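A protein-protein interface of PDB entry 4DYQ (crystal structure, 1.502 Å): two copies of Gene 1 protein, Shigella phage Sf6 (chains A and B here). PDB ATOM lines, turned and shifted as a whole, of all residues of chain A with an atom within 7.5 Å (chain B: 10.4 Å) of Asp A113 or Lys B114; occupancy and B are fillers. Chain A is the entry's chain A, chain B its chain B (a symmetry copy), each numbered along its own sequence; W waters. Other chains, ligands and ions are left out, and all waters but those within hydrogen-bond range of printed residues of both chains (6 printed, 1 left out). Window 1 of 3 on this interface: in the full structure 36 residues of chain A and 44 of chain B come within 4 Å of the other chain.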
ATOM      1  N   LYS A 100       2.762   7.613 -12.743  1.00  0.00           N
ATOM      2  CA  LYS A 100       1.734   8.651 -12.595  1.00  0.00           C
ATOM      3  C   LYS A 100       0.350   8.070 -12.849  1.00  0.00           C
ATOM      4  O   LYS A 100      -0.590   8.317 -12.087  1.00  0.00           O
ATOM      5  CB  LYS A 100       1.994   9.814 -13.557  1.00  0.00           C
ATOM      6  CG  LYS A 100       3.199  10.663 -13.166  1.00  0.00           C
ATOM      7  CD  LYS A 100       3.370  11.885 -14.057  1.00  0.00           C
ATOM      8  CE  LYS A 100       3.375  11.545 -15.508  1.00  0.00           C
ATOM      9  NZ  LYS A 100       3.588  12.771 -16.325  1.00  0.00           N
ATOM     10  N   TRP A 101       0.232   7.300 -13.919  1.00  0.00           N
ATOM     11  CA  TRP A 101      -1.036   6.692 -14.302  1.00  0.00           C
ATOM     12  C   TRP A 101      -1.494   5.737 -13.209  1.00  0.00           C
ATOM     13  O   TRP A 101      -2.655   5.754 -12.788  1.00  0.00           O
ATOM     14  CB  TRP A 101      -0.851   5.956 -15.636  1.00  0.00           C
ATOM     15  CG  TRP A 101      -2.085   5.377 -16.227  1.00  0.00           C
ATOM     16  CD1 TRP A 101      -2.936   5.987 -17.107  1.00  0.00           C
ATOM     17  CD2 TRP A 101      -2.601   4.070 -16.004  1.00  0.00           C
ATOM     18  NE1 TRP A 101      -3.956   5.135 -17.437  1.00  0.00           N
ATOM     19  CE2 TRP A 101      -3.778   3.947 -16.777  1.00  0.00           C
ATOM     20  CE3 TRP A 101      -2.190   2.987 -15.228  1.00  0.00           C
ATOM     21  CZ2 TRP A 101      -4.550   2.789 -16.786  1.00  0.00           C
ATOM     22  CZ3 TRP A 101      -2.963   1.819 -15.243  1.00  0.00           C
ATOM     23  CH2 TRP A 101      -4.126   1.741 -16.019  1.00  0.00           C
ATOM     24  N   LEU A 103      -0.656   5.696 -10.031  1.00  0.00           N
ATOM     25  CA  LEU A 103      -0.917   6.367  -8.756  1.00  0.00           C
ATOM     26  C   LEU A 103      -2.373   6.807  -8.669  1.00  0.00           C
ATOM     27  O   LEU A 103      -2.999   6.683  -7.617  1.00  0.00           O
ATOM     28  CB  LEU A 103       0.008   7.581  -8.595  1.00  0.00           C
ATOM     29  CG  LEU A 103       1.425   7.248  -8.127  1.00  0.00           C
ATOM     30  CD1 LEU A 103       2.313   8.475  -8.225  1.00  0.00           C
ATOM     31  CD2 LEU A 103       1.379   6.732  -6.719  1.00  0.00           C
ATOM     32  N   ALA A 104      -2.906   7.323  -9.770  1.00  0.00           N
ATOM     33  CA  ALA A 104      -4.283   7.787  -9.780  1.00  0.00           C
ATOM     34  C   ALA A 104      -5.247   6.662  -9.461  1.00  0.00           C
ATOM     35  O   ALA A 104      -6.296   6.885  -8.867  1.00  0.00           O
ATOM     36  CB  ALA A 104      -4.620   8.402 -11.126  1.00  0.00           C
ATOM     37  N   ARG A 105      -4.910   5.450  -9.875  1.00  0.00           N
ATOM     38  CA  ARG A 105      -5.784   4.312  -9.628  1.00  0.00           C
ATOM     39  C   ARG A 105      -5.576   3.705  -8.250  1.00  0.00           C
ATOM     40  O   ARG A 105      -6.505   3.146  -7.667  1.00  0.00           O
ATOM     41  CB  ARG A 105      -5.582   3.288 -10.724  1.00  0.00           C
ATOM     42  CG  ARG A 105      -6.239   3.778 -11.983  1.00  0.00           C
ATOM     43  CD  ARG A 105      -5.345   3.721 -13.162  1.00  0.00           C
ATOM     44  NE  ARG A 105      -6.084   4.198 -14.321  1.00  0.00           N
ATOM     45  CZ  ARG A 105      -5.960   5.400 -14.868  1.00  0.00           C
ATOM     46  NH1 ARG A 105      -5.095   6.290 -14.413  1.00  0.00           N
ATOM     47  NH2 ARG A 105      -6.701   5.682 -15.931  1.00  0.00           N
ATOM     48  N   MET A 106      -4.373   3.849  -7.706  1.00  0.00           N
ATOM     49  CA  MET A 106      -4.090   3.307  -6.382  1.00  0.00           C
ATOM     50  C   MET A 106      -4.723   4.158  -5.276  1.00  0.00           C
ATOM     51  O   MET A 106      -5.156   3.634  -4.250  1.00  0.00           O
ATOM     52  CB  MET A 106      -2.581   3.199  -6.185  1.00  0.00           C
ATOM     53  CG  MET A 106      -1.926   2.208  -7.121  1.00  0.00           C
ATOM     54  SD  MET A 106      -0.130   2.272  -7.083  1.00  0.00           S
ATOM     55  CE  MET A 106       0.215   1.400  -5.563  1.00  0.00           C
ATOM     56  N   ASN A 107      -4.753   5.471  -5.471  1.00  0.00           N
ATOM     57  CA  ASN A 107      -5.440   6.371  -4.548  1.00  0.00           C
ATOM     58  C   ASN A 107      -6.049   7.540  -5.319  1.00  0.00           C
ATOM     59  O   ASN A 107      -5.432   8.597  -5.471  1.00  0.00           O
ATOM     60  CB  ASN A 107      -4.493   6.872  -3.460  1.00  0.00           C
ATOM     61  CG  ASN A 107      -5.222   7.602  -2.352  1.00  0.00           C
ATOM     62  OD1 ASN A 107      -6.329   8.118  -2.542  1.00  0.00           O
ATOM     63  ND2 ASN A 107      -4.604   7.654  -1.187  1.00  0.00           N
ATOM     64  N   PRO A 108      -7.261   7.346  -5.849  1.00  0.00           N
ATOM     65  CA  PRO A 108      -7.895   8.372  -6.684  1.00  0.00           C
ATOM     66  C   PRO A 108      -8.092   9.716  -5.983  1.00  0.00           C
ATOM     67  O   PRO A 108      -7.923  10.763  -6.614  1.00  0.00           O
ATOM     68  CB  PRO A 108      -9.249   7.747  -7.033  1.00  0.00           C
ATOM     69  CG  PRO A 108      -9.028   6.283  -6.932  1.00  0.00           C
ATOM     70  CD  PRO A 108      -8.016   6.083  -5.848  1.00  0.00           C
ATOM     71  N   ARG A 109      -8.434   9.699  -4.702  1.00  0.00           N
ATOM     72  CA  ARG A 109      -8.683  10.939  -3.981  1.00  0.00           C
ATOM     73  C   ARG A 109      -7.429  11.792  -3.951  1.00  0.00           C
ATOM     74  O   ARG A 109      -7.487  13.013  -4.093  1.00  0.00           O
ATOM     75  CB  ARG A 109      -9.130  10.637  -2.550  1.00  0.00           C
ATOM     76  CG  ARG A 109      -9.823  11.801  -1.868  1.00  0.00           C
ATOM     77  CD  ARG A 109     -11.198  11.394  -1.341  1.00  0.00           C
ATOM     78  NE  ARG A 109     -11.108  10.469  -0.211  1.00  0.00           N
ATOM     79  CZ  ARG A 109     -11.731   9.295  -0.137  1.00  0.00           C
ATOM     80  NH1 ARG A 109     -12.509   8.873  -1.127  1.00  0.00           N
ATOM     81  NH2 ARG A 109     -11.578   8.535   0.941  1.00  0.00           N
ATOM     82  N   LYS A 110      -6.293  11.134  -3.768  1.00  0.00           N
ATOM     83  CA  LYS A 110      -5.031  11.808  -3.548  1.00  0.00           C
ATOM     84  C   LYS A 110      -4.327  12.117  -4.864  1.00  0.00           C
ATOM     85  O   LYS A 110      -3.802  13.217  -5.046  1.00  0.00           O
ATOM     86  CB  LYS A 110      -4.148  10.914  -2.693  1.00  0.00           C
ATOM     87  CG  LYS A 110      -2.934  11.551  -2.138  1.00  0.00           C
ATOM     88  CD  LYS A 110      -2.557  10.801  -0.874  1.00  0.00           C
ATOM     89  CE  LYS A 110      -1.416  11.440  -0.116  1.00  0.00           C
ATOM     90  NZ  LYS A 110      -1.136  10.634   1.105  1.00  0.00           N
ATOM     91  N   TYR A 111      -4.321  11.148  -5.780  1.00  0.00           N
ATOM     92  CA  TYR A 111      -3.468  11.235  -6.962  1.00  0.00           C
ATOM     93  C   TYR A 111      -4.205  11.358  -8.293  1.00  0.00           C
ATOM     94  O   TYR A 111      -3.572  11.433  -9.349  1.00  0.00           O
ATOM     95  CB  TYR A 111      -2.487  10.056  -6.993  1.00  0.00           C
ATOM     96  CG  TYR A 111      -1.557  10.043  -5.797  1.00  0.00           C
ATOM     97  CD1 TYR A 111      -0.691  11.105  -5.555  1.00  0.00           C
ATOM     98  CD2 TYR A 111      -1.542   8.977  -4.910  1.00  0.00           C
ATOM     99  CE1 TYR A 111       0.154  11.110  -4.466  1.00  0.00           C
ATOM    100  CE2 TYR A 111      -0.691   8.972  -3.819  1.00  0.00           C
ATOM    101  CZ  TYR A 111       0.150  10.049  -3.599  1.00  0.00           C
ATOM    102  OH  TYR A 111       1.005  10.073  -2.516  1.00  0.00           O
ATOM    103  N   GLY A 112      -5.533  11.406  -8.269  1.00  0.00           N
ATOM    104  CA  GLY A 112      -6.288  11.676  -9.474  1.00  0.00           C
ATOM    105  C   GLY A 112      -6.039  13.095  -9.984  1.00  0.00           C
ATOM    106  O   GLY A 112      -5.436  13.924  -9.296  1.00  0.00           O
ATOM    107  N   ASP A 113      -6.506  13.368 -11.193  1.00  0.00           N
ATOM    108  CA  ASP A 113      -6.385  14.691 -11.790  1.00  0.00           C
ATOM    109  C   ASP A 113      -7.191  15.696 -10.985  1.00  0.00           C
ATOM    110  O   ASP A 113      -8.184  15.344 -10.343  1.00  0.00           O
ATOM    111  CB  ASP A 113      -6.887  14.678 -13.234  1.00  0.00           C
ATOM    112  CG  ASP A 113      -5.886  14.103 -14.223  1.00  0.00           C
ATOM    113  OD1 ASP A 113      -4.736  13.762 -13.862  1.00  0.00           O
ATOM    114  OD2 ASP A 113      -6.277  14.018 -15.407  1.00  0.00           O
ATOM    115  N   LYS A 114      -6.762  16.950 -11.033  1.00  0.00           N
ATOM    116  CA  LYS A 114      -7.380  18.023 -10.272  1.00  0.00           C
ATOM    117  C   LYS A 114      -7.729  19.131 -11.234  1.00  0.00           C
ATOM    118  O   LYS A 114      -6.852  19.654 -11.920  1.00  0.00           O
ATOM    119  CB  LYS A 114      -6.407  18.559  -9.231  1.00  0.00           C
ATOM    120  CG  LYS A 114      -5.743  17.489  -8.399  1.00  0.00           C
ATOM    121  CD  LYS A 114      -6.725  16.826  -7.498  1.00  0.00           C
ATOM    122  CE  LYS A 114      -6.004  15.808  -6.644  1.00  0.00           C
ATOM    123  NZ  LYS A 114      -6.966  14.952  -5.960  1.00  0.00           N
ATOM    124  N   VAL A 115      -9.009  19.491 -11.293  1.00  0.00           N
ATOM    125  CA  VAL A 115      -9.471  20.539 -12.189  1.00  0.00           C
ATOM    126  C   VAL A 115     -10.428  21.437 -11.414  1.00  0.00           C
ATOM    127  O   VAL A 115     -11.247  20.956 -10.633  1.00  0.00           O
ATOM    128  CB  VAL A 115     -10.225  19.964 -13.401  1.00  0.00           C
ATOM    129  CG1 VAL A 115     -10.602  21.088 -14.357  1.00  0.00           C
ATOM    130  CG2 VAL A 115      -9.401  18.889 -14.111  1.00  0.00           C
ATOM    131  N   PHE B  72      -1.909  -4.855 -14.569  1.00  0.00           N
ATOM    132  CA  PHE B  72      -1.602  -3.636 -13.824  1.00  0.00           C
ATOM    133  C   PHE B  72      -0.228  -3.747 -13.188  1.00  0.00           C
ATOM    134  O   PHE B  72       0.519  -2.771 -13.134  1.00  0.00           O
ATOM    135  CB  PHE B  72      -2.679  -3.383 -12.761  1.00  0.00           C
ATOM    136  CG  PHE B  72      -2.491  -2.115 -11.979  1.00  0.00           C
ATOM    137  CD1 PHE B  72      -2.786  -0.895 -12.548  1.00  0.00           C
ATOM    138  CD2 PHE B  72      -2.049  -2.154 -10.669  1.00  0.00           C
ATOM    139  CE1 PHE B  72      -2.625   0.287 -11.828  1.00  0.00           C
ATOM    140  CE2 PHE B  72      -1.885  -0.970  -9.941  1.00  0.00           C
ATOM    141  CZ  PHE B  72      -2.176   0.235 -10.529  1.00  0.00           C
ATOM    142  N   LEU B 103      -6.927  -1.720 -19.818  1.00  0.00           N
ATOM    143  CA  LEU B 103      -7.303  -1.924 -18.419  1.00  0.00           C
ATOM    144  C   LEU B 103      -8.552  -1.130 -18.065  1.00  0.00           C
ATOM    145  O   LEU B 103      -9.417  -1.618 -17.331  1.00  0.00           O
ATOM    146  CB  LEU B 103      -6.160  -1.533 -17.466  1.00  0.00           C
ATOM    147  CG  LEU B 103      -5.218  -2.664 -17.043  1.00  0.00           C
ATOM    148  CD1 LEU B 103      -4.956  -3.647 -18.169  1.00  0.00           C
ATOM    149  CD2 LEU B 103      -3.921  -2.047 -16.523  1.00  0.00           C
ATOM    150  N   ALA B 104      -8.658   0.084 -18.590  1.00  0.00           N
ATOM    151  CA  ALA B 104      -9.804   0.921 -18.274  1.00  0.00           C
ATOM    152  C   ALA B 104     -11.080   0.282 -18.798  1.00  0.00           C
ATOM    153  O   ALA B 104     -12.148   0.462 -18.228  1.00  0.00           O
ATOM    154  CB  ALA B 104      -9.627   2.315 -18.843  1.00  0.00           C
ATOM    155  N   ASN B 107     -11.882  -3.148 -16.580  1.00  0.00           N
ATOM    156  CA  ASN B 107     -12.473  -2.823 -15.290  1.00  0.00           C
ATOM    157  C   ASN B 107     -12.552  -1.313 -15.116  1.00  0.00           C
ATOM    158  O   ASN B 107     -11.664  -0.696 -14.525  1.00  0.00           O
ATOM    159  CB  ASN B 107     -11.653  -3.448 -14.154  1.00  0.00           C
ATOM    160  CG  ASN B 107     -12.359  -3.365 -12.810  1.00  0.00           C
ATOM    161  OD1 ASN B 107     -13.208  -2.495 -12.587  1.00  0.00           O
ATOM    162  ND2 ASN B 107     -11.992  -4.254 -11.899  1.00  0.00           N
ATOM    163  N   PRO B 108     -13.622  -0.702 -15.639  1.00  0.00           N
ATOM    164  CA  PRO B 108     -13.733   0.760 -15.646  1.00  0.00           C
ATOM    165  C   PRO B 108     -13.731   1.376 -14.262  1.00  0.00           C
ATOM    166  O   PRO B 108     -13.152   2.449 -14.074  1.00  0.00           O
ATOM    167  CB  PRO B 108     -15.091   1.000 -16.306  1.00  0.00           C
ATOM    168  CG  PRO B 108     -15.316  -0.186 -17.152  1.00  0.00           C
ATOM    169  CD  PRO B 108     -14.689  -1.344 -16.426  1.00  0.00           C
ATOM    170  N   ARG B 109     -14.355   0.703 -13.302  1.00  0.00           N
ATOM    171  CA  ARG B 109     -14.479   1.250 -11.958  1.00  0.00           C
ATOM    172  C   ARG B 109     -13.113   1.373 -11.323  1.00  0.00           C
ATOM    173  O   ARG B 109     -12.816   2.351 -10.641  1.00  0.00           O
ATOM    174  CB  ARG B 109     -15.371   0.349 -11.112  1.00  0.00           C
ATOM    175  CG  ARG B 109     -16.181   1.078 -10.070  1.00  0.00           C
ATOM    176  CD  ARG B 109     -17.490   0.352  -9.837  1.00  0.00           C
ATOM    177  NE  ARG B 109     -17.279  -0.998  -9.318  1.00  0.00           N
ATOM    178  CZ  ARG B 109     -18.190  -1.967  -9.354  1.00  0.00           C
ATOM    179  NH1 ARG B 109     -19.381  -1.743  -9.897  1.00  0.00           N
ATOM    180  NH2 ARG B 109     -17.907  -3.164  -8.856  1.00  0.00           N
ATOM    181  N   LYS B 110     -12.262   0.390 -11.573  1.00  0.00           N
ATOM    182  CA  LYS B 110     -10.953   0.363 -10.952  1.00  0.00           C
ATOM    183  C   LYS B 110      -9.903   1.140 -11.746  1.00  0.00           C
ATOM    184  O   LYS B 110      -9.082   1.864 -11.172  1.00  0.00           O
ATOM    185  CB  LYS B 110     -10.506  -1.077 -10.805  1.00  0.00           C
ATOM    186  CG  LYS B 110      -9.264  -1.239 -10.005  1.00  0.00           C
ATOM    187  CD  LYS B 110      -9.164  -2.667  -9.518  1.00  0.00           C
ATOM    188  CE  LYS B 110      -7.983  -2.842  -8.605  1.00  0.00           C
ATOM    189  NZ  LYS B 110      -7.891  -4.254  -8.157  1.00  0.00           N
ATOM    190  N   TYR B 111      -9.918   0.981 -13.065  1.00  0.00           N
ATOM    191  CA  TYR B 111      -8.812   1.455 -13.881  1.00  0.00           C
ATOM    192  C   TYR B 111      -9.161   2.582 -14.850  1.00  0.00           C
ATOM    193  O   TYR B 111      -8.310   3.015 -15.610  1.00  0.00           O
ATOM    194  CB  TYR B 111      -8.183   0.281 -14.650  1.00  0.00           C
ATOM    195  CG  TYR B 111      -7.594  -0.781 -13.749  1.00  0.00           C
ATOM    196  CD1 TYR B 111      -6.581  -0.475 -12.846  1.00  0.00           C
ATOM    197  CD2 TYR B 111      -8.047  -2.090 -13.805  1.00  0.00           C
ATOM    198  CE1 TYR B 111      -6.041  -1.445 -12.010  1.00  0.00           C
ATOM    199  CE2 TYR B 111      -7.510  -3.072 -12.972  1.00  0.00           C
ATOM    200  CZ  TYR B 111      -6.511  -2.732 -12.083  1.00  0.00           C
ATOM    201  OH  TYR B 111      -5.974  -3.692 -11.254  1.00  0.00           O
ATOM    202  N   GLY B 112     -10.396   3.066 -14.812  1.00  0.00           N
ATOM    203  CA  GLY B 112     -10.747   4.277 -15.536  1.00  0.00           C
ATOM    204  C   GLY B 112      -9.994   5.493 -15.014  1.00  0.00           C
ATOM    205  O   GLY B 112      -9.370   5.452 -13.948  1.00  0.00           O
ATOM    206  N   ASP B 113     -10.070   6.592 -15.763  1.00  0.00           N
ATOM    207  CA  ASP B 113      -9.441   7.838 -15.352  1.00  0.00           C
ATOM    208  C   ASP B 113     -10.112   8.357 -14.082  1.00  0.00           C
ATOM    209  O   ASP B 113     -11.288   8.074 -13.847  1.00  0.00           O
ATOM    210  CB  ASP B 113      -9.576   8.905 -16.448  1.00  0.00           C
ATOM    211  CG  ASP B 113      -8.595   8.725 -17.597  1.00  0.00           C
ATOM    212  OD1 ASP B 113      -7.701   7.855 -17.543  1.00  0.00           O
ATOM    213  OD2 ASP B 113      -8.717   9.506 -18.563  1.00  0.00           O
ATOM    214  N   LYS B 114      -9.374   9.138 -13.293  1.00  0.00           N
ATOM    215  CA  LYS B 114      -9.847   9.658 -12.013  1.00  0.00           C
ATOM    216  C   LYS B 114      -9.650  11.156 -12.035  1.00  0.00           C
ATOM    217  O   LYS B 114      -8.533  11.623 -12.229  1.00  0.00           O
ATOM    218  CB  LYS B 114      -9.044   9.045 -10.854  1.00  0.00           C
ATOM    219  CG  LYS B 114      -8.896   7.536 -10.948  1.00  0.00           C
ATOM    220  CD  LYS B 114     -10.211   6.852 -10.741  1.00  0.00           C
ATOM    221  CE  LYS B 114     -10.003   5.347 -10.746  1.00  0.00           C
ATOM    222  NZ  LYS B 114     -11.274   4.620 -10.748  1.00  0.00           N
ATOM    223  N   VAL B 115     -10.733  11.919 -11.878  1.00  0.00           N
ATOM    224  CA  VAL B 115     -10.657  13.371 -11.901  1.00  0.00           C
ATOM    225  C   VAL B 115     -11.491  13.894 -10.750  1.00  0.00           C
ATOM    226  O   VAL B 115     -12.579  13.373 -10.490  1.00  0.00           O
ATOM    227  CB  VAL B 115     -11.225  13.951 -13.211  1.00  0.00           C
ATOM    228  CG1 VAL B 115     -11.055  15.464 -13.244  1.00  0.00           C
ATOM    229  CG2 VAL B 115     -10.565  13.316 -14.423  1.00  0.00           C
ATOM    230  N   THR B 116     -10.973  14.893 -10.042  1.00  0.00           N
ATOM    231  CA  THR B 116     -11.781  15.653  -9.087  1.00  0.00           C
ATOM    232  C   THR B 116     -12.032  17.026  -9.694  1.00  0.00           C
ATOM    233  O   THR B 116     -11.079  17.754  -9.986  1.00  0.00           O
ATOM    234  CB  THR B 116     -11.079  15.818  -7.737  1.00  0.00           C
ATOM    235  OG1 THR B 116     -10.807  14.521  -7.180  1.00  0.00           O
ATOM    236  CG2 THR B 116     -11.955  16.630  -6.765  1.00  0.00           C
ATOM    237  N   ASN B 117     -13.301  17.361  -9.919  1.00  0.00           N
ATOM    238  CA  ASN B 117     -13.685  18.651 -10.476  1.00  0.00           C
ATOM    239  C   ASN B 117     -14.251  19.528  -9.377  1.00  0.00           C
ATOM    240  O   ASN B 117     -15.303  19.219  -8.821  1.00  0.00           O
ATOM    241  CB  ASN B 117     -14.748  18.485 -11.562  1.00  0.00           C
ATOM    242  CG  ASN B 117     -14.262  17.689 -12.752  1.00  0.00           C
ATOM    243  OD1 ASN B 117     -13.733  18.236 -13.742  1.00  0.00           O
ATOM    244  ND2 ASN B 117     -14.457  16.401 -12.686  1.00  0.00           N
ATOM    245  N   GLU B 118     -13.539  20.605  -9.059  1.00  0.00           N
ATOM    246  CA  GLU B 118     -14.037  21.641  -8.167  1.00  0.00           C
ATOM    247  C   GLU B 118     -14.875  22.579  -9.015  1.00  0.00           C
ATOM    248  O   GLU B 118     -14.340  23.300  -9.858  1.00  0.00           O
ATOM    249  CB  GLU B 118     -12.869  22.389  -7.516  1.00  0.00           C
ATOM    250  CG  GLU B 118     -13.304  23.538  -6.602  1.00  0.00           C
ATOM    251  CD  GLU B 118     -12.161  24.467  -6.188  1.00  0.00           C
ATOM    252  OE1 GLU B 118     -11.111  24.502  -6.857  1.00  0.00           O
ATOM    253  OE2 GLU B 118     -12.319  25.182  -5.178  1.00  0.00           O
HETATM  254  O   HOH W   1     -10.399  11.616  -8.030  1.00  0.00           O
HETATM  255  O   HOH W   2      -5.649   7.485 -19.016  1.00  0.00           O
HETATM  256  O   HOH W   3      -8.600   5.344 -18.615  1.00  0.00           O
HETATM  257  O   HOH W   4      -8.981   2.747  -8.662  1.00  0.00           O
HETATM  258  O   HOH W   5     -10.223  14.568  -3.985  1.00  0.00           O
HETATM  259  O   HOH W   6      -9.768  19.513  -7.922  1.00  0.00           O
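Among the printed residues, merely in contact across the chains: Trp A101 with Phe B72, Trp A101 with Leu B103, Trp A101 with Tyr B111, Ala A104 with Lys B114, Arg A105 with Lys B110, Met A106 with Phe B72, Pro A108 with Lys B114, Gly A112 with Lys B114, Asp A113 with Val B115, Lys A114 with Thr B116, Val A115 with Val B115 and Val A115 with Asn B117.
Water W2 bridges the side-chain carboxylate of Asp B113 and the indole nitrogen of Trp A101.
Water W4 lies within hydrogen-bond range of the backbone carbonyl oxygen (O) of Lys B110 (2.7 Å) and the backbone carbonyl oxygen (O) of Arg A105 (2.7 Å).
Water W3 lies within hydrogen-bond range of OD1 of Asp B113 (2.9 Å) and NH2 of Arg A105 (3.3 Å).
Water W1 lies within hydrogen-bond range of O of Pro A108 (3.0 Å) and OG1 of Thr B116 (3.1 Å).
Water W6 bridges O of Thr B116 (3.0 Å) and O of Val A115 (3.4 Å).
Water W5 lies within hydrogen-bond range of the backbone carbonyl oxygen (O) of Arg A109 (3.1 Å) and the side-chain hydroxyl (OG1) of Thr B116 (3.2 Å).
Asp A113 touches three residues of chain B.
Of chain A, only Ala A104 (3.4 Å), Pro A108 (3.9 Å), Gly A112 (3.6 Å) and Asp A113 (2.9 Å) come within 4 Å of Lys B114.
Gly A112 touches one residue of chain B.
Printed residues of chain A within 4 Å of Tyr B111: Trp A101 and Arg A105.
Of the printed residues of chain B, Trp A101 touches Phe B72 (3.8 Å), Leu B103 (3.8 Å) and Tyr B111 (3.9 Å).
Of the printed residues of chain A, Lys B110 touches Arg A105.
Printed residues of chain A within 4 Å of Thr B116: Asp A113 (2.8 Å), Lys A114 (3.7 Å) and Val A115 (3.0 Å).
Printed residues of chain B within 4 Å of Met A106: Phe B72.
Leu A103 touches none of the printed residues of chain B.
The side-chain amide oxygen (OD1) of Asn B107 sits at hydrogen-bond distance from the backbone NH (N) of Lys B110, 3.2 Å away.
The backbone carbonyl oxygen (O) of Trp A101 lies within hydrogen-bond range of the guanidinium group (NH1) of Arg A105 (3.0 Å).
O of Arg B109 lies within hydrogen-bond range of NZ of Lys B114.
The backbone carbonyl oxygen (O) of Arg A109 lies within hydrogen-bond range of the side-chain amino group (NZ) of Lys A114, at 2.7 Å.
The backbone carbonyl oxygen (O) of Lys B114 sits at hydrogen-bond distance from the backbone NH (N) of Asp A113 (2.9 Å).
The backbone carbonyl oxygen of Gly B112 lies within hydrogen-bond range of the guanidinium group of Arg A105 (3.3 Å).
The backbone carbonyl oxygen (O) of Val A115 sits at hydrogen-bond distance from the backbone NH (N) of Glu B118 (2.8 Å).
NE of Arg A105 lies within hydrogen-bond range of O of Tyr B111 (2.8 Å).
The backbone carbonyl oxygen (O) of Thr B116 is in hydrogen-bond range of the backbone NH (N) of Val A115 (3.0 Å).
The side-chain carboxylate of Asp B113 is in salt-bridge range of the guanidinium group of Arg A105 (2.9 Å).
The backbone carbonyl oxygen (O) of Asp A113 lies within hydrogen-bond range of the backbone NH (N) of Thr B116.
Ala A104 touches Lys B114, but with the chains exchanged Lys A114 does not touch Ala B104 (16.8 Å).
Gly A112 touches Lys B114, but with the chains exchanged Lys A114 does not touch Gly B112 (12.1 Å).
Asp A113 touches Lys B114, but with the chains exchanged Lys A114 does not touch Asp B113 (9.7 Å).
Asp A113 touches Val B115, but with the chains exchanged Val A115 does not touch Asp B113 (10.3 Å).
Of the 19 pairs that touch across the chains among the printed residues, 1 has its exchanged pair printed and touching as well.
Hydrophobic or aromatic side chains of chain A within 4 Å of the printed part of chain B: Trp A101, Met A106, Pro A108 and Val A115.
Hydrophobic or aromatic side chains of chain B that line the printed part of chain A: Phe B72, Leu B103 and Val B115.
Along chain B the printed residues that touch a printed residue of chain A span positions 72 to 118.
Among the printed residues, Asp or Glu carboxylates within 4 Å of a Lys or Arg side-chain nitrogen of the other chain: Arg A105 with Asp B113.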
